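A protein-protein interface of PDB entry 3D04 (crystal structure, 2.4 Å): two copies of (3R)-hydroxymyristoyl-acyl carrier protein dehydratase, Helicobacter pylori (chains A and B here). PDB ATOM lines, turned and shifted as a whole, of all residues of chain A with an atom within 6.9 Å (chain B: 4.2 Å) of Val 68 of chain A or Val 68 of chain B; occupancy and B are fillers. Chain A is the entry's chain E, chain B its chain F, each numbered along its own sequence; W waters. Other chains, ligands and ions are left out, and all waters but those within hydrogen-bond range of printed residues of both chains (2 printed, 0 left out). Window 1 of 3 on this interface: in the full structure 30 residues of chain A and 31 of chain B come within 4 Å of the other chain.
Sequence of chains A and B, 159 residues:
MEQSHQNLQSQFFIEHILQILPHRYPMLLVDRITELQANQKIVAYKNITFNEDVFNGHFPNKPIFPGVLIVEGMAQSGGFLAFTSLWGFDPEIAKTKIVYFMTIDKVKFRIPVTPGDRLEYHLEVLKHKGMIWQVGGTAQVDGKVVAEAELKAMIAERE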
ATOM      1  N   MET A  27       8.510 -16.012  28.522  1.00  0.00           N
ATOM      2  CA  MET A  27       9.404 -17.033  27.968  1.00  0.00           C
ATOM      3  C   MET A  27       9.683 -18.236  28.886  1.00  0.00           C
ATOM      4  O   MET A  27      10.594 -19.029  28.616  1.00  0.00           O
ATOM      5  CB  MET A  27      10.714 -16.393  27.490  1.00  0.00           C
ATOM      6  CG  MET A  27      10.603 -15.679  26.143  1.00  0.00           C
ATOM      7  SD  MET A  27      10.210 -16.776  24.750  1.00  0.00           S
ATOM      8  CE  MET A  27      11.748 -17.690  24.606  1.00  0.00           C
ATOM      9  N   LEU A  29       8.251 -21.603  29.634  1.00  0.00           N
ATOM     10  CA  LEU A  29       7.349 -22.434  28.832  1.00  0.00           C
ATOM     11  C   LEU A  29       7.274 -23.878  29.330  1.00  0.00           C
ATOM     12  O   LEU A  29       7.002 -24.803  28.565  1.00  0.00           O
ATOM     13  CB  LEU A  29       7.747 -22.368  27.341  1.00  0.00           C
ATOM     14  CG  LEU A  29       7.888 -20.975  26.702  1.00  0.00           C
ATOM     15  CD1 LEU A  29       8.261 -21.064  25.227  1.00  0.00           C
ATOM     16  CD2 LEU A  29       6.628 -20.120  26.879  1.00  0.00           C
ATOM     17  N   PHE A  65       0.013 -22.846  18.370  1.00  0.00           N
ATOM     18  CA  PHE A  65       1.210 -22.679  19.186  1.00  0.00           C
ATOM     19  C   PHE A  65       2.469 -22.827  18.325  1.00  0.00           C
ATOM     20  O   PHE A  65       2.660 -23.864  17.690  1.00  0.00           O
ATOM     21  CB  PHE A  65       1.218 -23.651  20.378  1.00  0.00           C
ATOM     22  CG  PHE A  65       2.211 -23.282  21.455  1.00  0.00           C
ATOM     23  CD1 PHE A  65       1.973 -22.201  22.301  1.00  0.00           C
ATOM     24  CD2 PHE A  65       3.394 -24.007  21.613  1.00  0.00           C
ATOM     25  CE1 PHE A  65       2.897 -21.854  23.295  1.00  0.00           C
ATOM     26  CE2 PHE A  65       4.324 -23.660  22.594  1.00  0.00           C
ATOM     27  CZ  PHE A  65       4.075 -22.584  23.437  1.00  0.00           C
ATOM     28  N   PRO A  66       3.315 -21.776  18.279  1.00  0.00           N
ATOM     29  CA  PRO A  66       4.469 -21.775  17.370  1.00  0.00           C
ATOM     30  C   PRO A  66       5.410 -22.959  17.606  1.00  0.00           C
ATOM     31  O   PRO A  66       5.759 -23.260  18.752  1.00  0.00           O
ATOM     32  CB  PRO A  66       5.168 -20.439  17.674  1.00  0.00           C
ATOM     33  CG  PRO A  66       4.112 -19.579  18.294  1.00  0.00           C
ATOM     34  CD  PRO A  66       3.239 -20.530  19.071  1.00  0.00           C
ATOM     35  N   GLY A  67       5.783 -23.629  16.515  1.00  0.00           N
ATOM     36  CA  GLY A  67       6.738 -24.724  16.545  1.00  0.00           C
ATOM     37  C   GLY A  67       8.054 -24.397  17.238  1.00  0.00           C
ATOM     38  O   GLY A  67       8.581 -25.223  17.987  1.00  0.00           O
ATOM     39  N   VAL A  68       8.584 -23.195  16.998  1.00  0.00           N
ATOM     40  CA  VAL A  68       9.837 -22.757  17.632  1.00  0.00           C
ATOM     41  C   VAL A  68       9.728 -22.643  19.156  1.00  0.00           C
ATOM     42  O   VAL A  68      10.733 -22.733  19.853  1.00  0.00           O
ATOM     43  CB  VAL A  68      10.410 -21.432  17.029  1.00  0.00           C
ATOM     44  CG1 VAL A  68      10.742 -21.608  15.547  1.00  0.00           C
ATOM     45  CG2 VAL A  68       9.475 -20.236  17.270  1.00  0.00           C
ATOM     46  N   LEU A  69       8.514 -22.465  19.670  1.00  0.00           N
ATOM     47  CA  LEU A  69       8.306 -22.373  21.114  1.00  0.00           C
ATOM     48  C   LEU A  69       8.157 -23.749  21.770  1.00  0.00           C
ATOM     49  O   LEU A  69       8.420 -23.903  22.965  1.00  0.00           O
ATOM     50  CB  LEU A  69       7.126 -21.456  21.450  1.00  0.00           C
ATOM     51  CG  LEU A  69       7.265 -19.976  21.057  1.00  0.00           C
ATOM     52  CD1 LEU A  69       6.090 -19.164  21.597  1.00  0.00           C
ATOM     53  CD2 LEU A  69       8.605 -19.358  21.495  1.00  0.00           C
ATOM     54  N   ILE A  70       7.732 -24.732  20.976  1.00  0.00           N
ATOM     55  CA  ILE A  70       7.736 -26.135  21.375  1.00  0.00           C
ATOM     56  C   ILE A  70       9.177 -26.578  21.606  1.00  0.00           C
ATOM     57  O   ILE A  70       9.486 -27.174  22.634  1.00  0.00           O
ATOM     58  CB  ILE A  70       7.079 -27.035  20.302  1.00  0.00           C
ATOM     59  CG1 ILE A  70       5.615 -26.634  20.078  1.00  0.00           C
ATOM     60  CG2 ILE A  70       7.202 -28.508  20.690  1.00  0.00           C
ATOM     61  CD1 ILE A  70       4.895 -27.433  19.014  1.00  0.00           C
ATOM     62  N   VAL A  71      10.050 -26.260  20.652  1.00  0.00           N
ATOM     63  CA  VAL A  71      11.492 -26.510  20.770  1.00  0.00           C
ATOM     64  C   VAL A  71      12.087 -25.792  21.981  1.00  0.00           C
ATOM     65  O   VAL A  71      12.856 -26.387  22.745  1.00  0.00           O
ATOM     66  CB  VAL A  71      12.256 -26.112  19.477  1.00  0.00           C
ATOM     67  CG1 VAL A  71      13.775 -26.298  19.649  1.00  0.00           C
ATOM     68  CG2 VAL A  71      11.748 -26.927  18.278  1.00  0.00           C
ATOM     69  N   GLU A  72      11.724 -24.520  22.146  1.00  0.00           N
ATOM     70  CA  GLU A  72      12.103 -23.732  23.320  1.00  0.00           C
ATOM     71  C   GLU A  72      11.727 -24.416  24.641  1.00  0.00           C
ATOM     72  O   GLU A  72      12.565 -24.521  25.538  1.00  0.00           O
ATOM     73  CB  GLU A  72      11.498 -22.319  23.238  1.00  0.00           C
ATOM     74  CG  GLU A  72      11.824 -21.397  24.415  1.00  0.00           C
ATOM     75  CD  GLU A  72      13.304 -21.095  24.573  1.00  0.00           C
ATOM     76  OE1 GLU A  72      14.026 -21.064  23.560  1.00  0.00           O
ATOM     77  OE2 GLU A  72      13.751 -20.867  25.720  1.00  0.00           O
ATOM     78  N   GLY A  73      10.480 -24.879  24.753  1.00  0.00           N
ATOM     79  CA  GLY A  73      10.022 -25.591  25.942  1.00  0.00           C
ATOM     80  C   GLY A  73      10.751 -26.904  26.189  1.00  0.00           C
ATOM     81  O   GLY A  73      10.998 -27.272  27.340  1.00  0.00           O
ATOM     82  N   ALA A  75      13.870 -27.401  25.234  1.00  0.00           N
ATOM     83  CA  ALA A  75      15.178 -26.931  25.694  1.00  0.00           C
ATOM     84  C   ALA A  75      15.166 -26.577  27.176  1.00  0.00           C
ATOM     85  O   ALA A  75      16.109 -26.891  27.903  1.00  0.00           O
ATOM     86  CB  ALA A  75      15.625 -25.740  24.882  1.00  0.00           C
ATOM     87  N   PHE A 101      21.187 -21.555  23.823  1.00  0.00           N
ATOM     88  CA  PHE A 101      21.115 -22.493  22.715  1.00  0.00           C
ATOM     89  C   PHE A 101      22.431 -22.480  21.959  1.00  0.00           C
ATOM     90  O   PHE A 101      22.978 -21.417  21.652  1.00  0.00           O
ATOM     91  CB  PHE A 101      20.007 -22.082  21.744  1.00  0.00           C
ATOM     92  CG  PHE A 101      18.781 -22.929  21.823  1.00  0.00           C
ATOM     93  CD1 PHE A 101      18.815 -24.257  21.416  1.00  0.00           C
ATOM     94  CD2 PHE A 101      17.586 -22.396  22.288  1.00  0.00           C
ATOM     95  CE1 PHE A 101      17.676 -25.047  21.481  1.00  0.00           C
ATOM     96  CE2 PHE A 101      16.442 -23.179  22.356  1.00  0.00           C
ATOM     97  CZ  PHE A 101      16.486 -24.505  21.947  1.00  0.00           C
ATOM     98  N   ILE A 104      20.511 -26.735  17.082  1.00  0.00           N
ATOM     99  CA  ILE A 104      19.226 -27.402  16.946  1.00  0.00           C
ATOM    100  C   ILE A 104      19.311 -28.267  15.684  1.00  0.00           C
ATOM    101  O   ILE A 104      19.742 -27.793  14.632  1.00  0.00           O
ATOM    102  CB  ILE A 104      18.036 -26.404  16.807  1.00  0.00           C
ATOM    103  CG1 ILE A 104      18.038 -25.344  17.919  1.00  0.00           C
ATOM    104  CG2 ILE A 104      16.710 -27.157  16.781  1.00  0.00           C
ATOM    105  CD1 ILE A 104      16.986 -24.238  17.745  1.00  0.00           C
ATOM    106  N   PHE A 109       7.926 -31.323  12.801  1.00  0.00           N
ATOM    107  CA  PHE A 109       6.611 -31.040  13.383  1.00  0.00           C
ATOM    108  C   PHE A 109       5.556 -31.860  12.650  1.00  0.00           C
ATOM    109  O   PHE A 109       5.453 -31.789  11.427  1.00  0.00           O
ATOM    110  CB  PHE A 109       6.275 -29.549  13.273  1.00  0.00           C
ATOM    111  CG  PHE A 109       7.296 -28.642  13.898  1.00  0.00           C
ATOM    112  CD1 PHE A 109       8.214 -27.963  13.107  1.00  0.00           C
ATOM    113  CD2 PHE A 109       7.337 -28.466  15.276  1.00  0.00           C
ATOM    114  CE1 PHE A 109       9.158 -27.114  13.684  1.00  0.00           C
ATOM    115  CE2 PHE A 109       8.281 -27.630  15.858  1.00  0.00           C
ATOM    116  CZ  PHE A 109       9.185 -26.948  15.060  1.00  0.00           C
ATOM    117  N   PRO B  66      15.918 -14.434  21.719  1.00  0.00           N
ATOM    118  CA  PRO B  66      15.887 -15.899  21.681  1.00  0.00           C
ATOM    119  C   PRO B  66      16.329 -16.502  20.348  1.00  0.00           C
ATOM    120  O   PRO B  66      15.910 -16.050  19.271  1.00  0.00           O
ATOM    121  CB  PRO B  66      14.416 -16.228  21.997  1.00  0.00           C
ATOM    122  CG  PRO B  66      13.929 -15.038  22.770  1.00  0.00           C
ATOM    123  CD  PRO B  66      14.600 -13.877  22.088  1.00  0.00           C
ATOM    124  N   GLY B  67      17.186 -17.515  20.443  1.00  0.00           N
ATOM    125  CA  GLY B  67      17.669 -18.240  19.279  1.00  0.00           C
ATOM    126  C   GLY B  67      16.543 -18.784  18.416  1.00  0.00           C
ATOM    127  O   GLY B  67      16.636 -18.773  17.185  1.00  0.00           O
ATOM    128  N   VAL B  68      15.472 -19.253  19.057  1.00  0.00           N
ATOM    129  CA  VAL B  68      14.332 -19.824  18.331  1.00  0.00           C
ATOM    130  C   VAL B  68      13.579 -18.763  17.518  1.00  0.00           C
ATOM    131  O   VAL B  68      12.969 -19.073  16.498  1.00  0.00           O
ATOM    132  CB  VAL B  68      13.369 -20.631  19.260  1.00  0.00           C
ATOM    133  CG1 VAL B  68      14.091 -21.824  19.875  1.00  0.00           C
ATOM    134  CG2 VAL B  68      12.753 -19.755  20.347  1.00  0.00           C
ATOM    135  N   LEU B  69      13.653 -17.512  17.975  1.00  0.00           N
ATOM    136  CA  LEU B  69      13.010 -16.379  17.315  1.00  0.00           C
ATOM    137  C   LEU B  69      13.849 -15.830  16.169  1.00  0.00           C
ATOM    138  O   LEU B  69      13.311 -15.199  15.259  1.00  0.00           O
ATOM    139  CB  LEU B  69      12.691 -15.276  18.327  1.00  0.00           C
ATOM    140  CG  LEU B  69      11.656 -15.580  19.420  1.00  0.00           C
ATOM    141  CD1 LEU B  69      11.296 -14.296  20.138  1.00  0.00           C
ATOM    142  CD2 LEU B  69      10.399 -16.253  18.846  1.00  0.00           C
ATOM    143  N   ILE B  70      15.161 -16.069  16.222  1.00  0.00           N
ATOM    144  CA  ILE B  70      16.043 -15.832  15.080  1.00  0.00           C
ATOM    145  C   ILE B  70      15.644 -16.778  13.950  1.00  0.00           C
ATOM    146  O   ILE B  70      15.475 -16.352  12.808  1.00  0.00           O
ATOM    147  CB  ILE B  70      17.550 -16.034  15.434  1.00  0.00           C
ATOM    148  CG1 ILE B  70      18.002 -15.026  16.504  1.00  0.00           C
ATOM    149  CG2 ILE B  70      18.436 -15.895  14.175  1.00  0.00           C
ATOM    150  CD1 ILE B  70      19.383 -15.293  17.068  1.00  0.00           C
ATOM    151  N   VAL B  71      15.484 -18.055  14.287  1.00  0.00           N
ATOM    152  CA  VAL B  71      15.035 -19.074  13.334  1.00  0.00           C
ATOM    153  C   VAL B  71      13.629 -18.750  12.781  1.00  0.00           C
ATOM    154  O   VAL B  71      13.394 -18.870  11.576  1.00  0.00           O
ATOM    155  CB  VAL B  71      15.066 -20.504  13.957  1.00  0.00           C
ATOM    156  CG1 VAL B  71      14.590 -21.562  12.943  1.00  0.00           C
ATOM    157  CG2 VAL B  71      16.458 -20.840  14.464  1.00  0.00           C
ATOM    158  N   GLU B  72      12.712 -18.346  13.661  1.00  0.00           N
ATOM    159  CA  GLU B  72      11.369 -17.924  13.253  1.00  0.00           C
ATOM    160  C   GLU B  72      11.411 -16.770  12.238  1.00  0.00           C
ATOM    161  O   GLU B  72      10.742 -16.821  11.199  1.00  0.00           O
ATOM    162  CB  GLU B  72      10.523 -17.563  14.487  1.00  0.00           C
ATOM    163  CG  GLU B  72       9.088 -17.113  14.201  1.00  0.00           C
ATOM    164  CD  GLU B  72       8.197 -18.200  13.588  1.00  0.00           C
ATOM    165  OE1 GLU B  72       8.379 -19.403  13.874  1.00  0.00           O
ATOM    166  OE2 GLU B  72       7.298 -17.837  12.811  1.00  0.00           O
ATOM    167  N   PHE B 101       5.497 -24.588  10.038  1.00  0.00           N
ATOM    168  CA  PHE B 101       6.826 -25.181  10.114  1.00  0.00           C
ATOM    169  C   PHE B 101       6.722 -26.689   9.927  1.00  0.00           C
ATOM    170  O   PHE B 101       5.870 -27.333  10.547  1.00  0.00           O
ATOM    171  CB  PHE B 101       7.440 -24.901  11.482  1.00  0.00           C
ATOM    172  CG  PHE B 101       8.613 -23.969  11.453  1.00  0.00           C
ATOM    173  CD1 PHE B 101       8.525 -22.705  12.027  1.00  0.00           C
ATOM    174  CD2 PHE B 101       9.817 -24.361  10.870  1.00  0.00           C
ATOM    175  CE1 PHE B 101       9.615 -21.841  12.017  1.00  0.00           C
ATOM    176  CE2 PHE B 101      10.911 -23.502  10.849  1.00  0.00           C
ATOM    177  CZ  PHE B 101      10.811 -22.241  11.430  1.00  0.00           C
HETATM  178  O   HOH W   1       7.228 -21.393  15.010  1.00  0.00           O
HETATM  179  O   HOH W   2      15.536 -19.458  22.324  1.00  0.00           O
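Val 68 of chain A touches three residues of chain B.
Val 68 of chain B touches just these residues of chain A: Val 68 (3.4 Å), Glu 72 (3.7 Å) and Phe 101 (3.7 Å).
Of the printed residues of chain A, Phe 101 of chain B touches Val 68 (3.7 Å) and Phe 109 (3.5 Å).
Printed residues of chain B within 4 Å of Met 27 of chain A: Pro 66.
Printed residues of chain A within 4 Å of Glu 72 of chain B: Val 68.
Printed residues of chain A within 4 Å of Pro 66 of chain B: Met 27.
Of the printed residues of chain B, Phe 109 of chain A touches Phe 101.
Ile 70 of chain B touches none of the printed residues of chain A.
Val 71 of chain B touches none of the printed residues of chain A.
The nearest printed residue of chain B that does not touch Val 68 of chain A is Leu 69 of chain B (4.4 Å).
The nearest printed residue of chain A that does not touch Val 68 of chain B is Leu 69 of chain A (4.3 Å).
The nearest printed residue of chain A that does not touch Pro 66 of chain B is Glu 72 of chain A (5.1 Å).
Water W2 lies within hydrogen-bond range of the side-chain carboxylate of Glu 72 of chain A (2.5 Å), the backbone NH of Gly 67 of chain B (3.2 Å) and the backbone NH of Val 68 of chain B (3.3 Å).
Water W1 lies within hydrogen-bond range of the side-chain carboxylate (OE1) of Glu 72 of chain B, the backbone NH (N) of Val 68 of chain A and the backbone NH (N) of Gly 67 of chain A.
Of the 8 printed residues of chain B, 4 touch a printed residue of chain A.
Along chain B the printed residues that touch a printed residue of chain A span positions 66 to 101.
Printed residues of chain A that touch a printed residue of chain B: Met 27, Val 68, Glu 72, Phe 101 and Phe 109.
Hydrophobic or aromatic side chains of chain A within 4 Å of the printed part of chain B: Met 27, Val 68, Phe 101 and Phe 109.
Along chain A the printed residues that touch a printed residue of chain B span positions 27 to 109.
Among the printed residues, no Asp or Glu carboxylate lies within 4 Å of a Lys or Arg side-chain nitrogen of the other chain.
Val 68 of chain A touches its own counterpart, Val 68 of chain B.
Val 68 of chain A touches Glu 72 of chain B, and with the chains exchanged Glu 72 of chain A touches Val 68 of chain B.
Val 68 of chain A touches Phe 101 of chain B, and with the chains exchanged Phe 101 of chain A touches Val 68 of chain B.
Of the 7 pairs that touch across the chains among the printed residues, 5 have their exchanged pair printed and touching as well.
Among the printed residues, merely in contact across the chains: Val 68 of chain A with Val 68 of chain B (3.4 Å), Phe 109 of chain A with Phe 101 of chain B (3.5 Å), Val 68 of chain A with Glu 72 of chain B (3.6 Å), Phe 101 of chain A with Val 68 of chain B (3.7 Å), Glu 72 of chain A with Val 68 of chain B (3.7 Å), Val 68 of chain A with Phe 101 of chain B (3.7 Å) and Met 27 of chain A with Pro 66 of chain B (3.9 Å).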
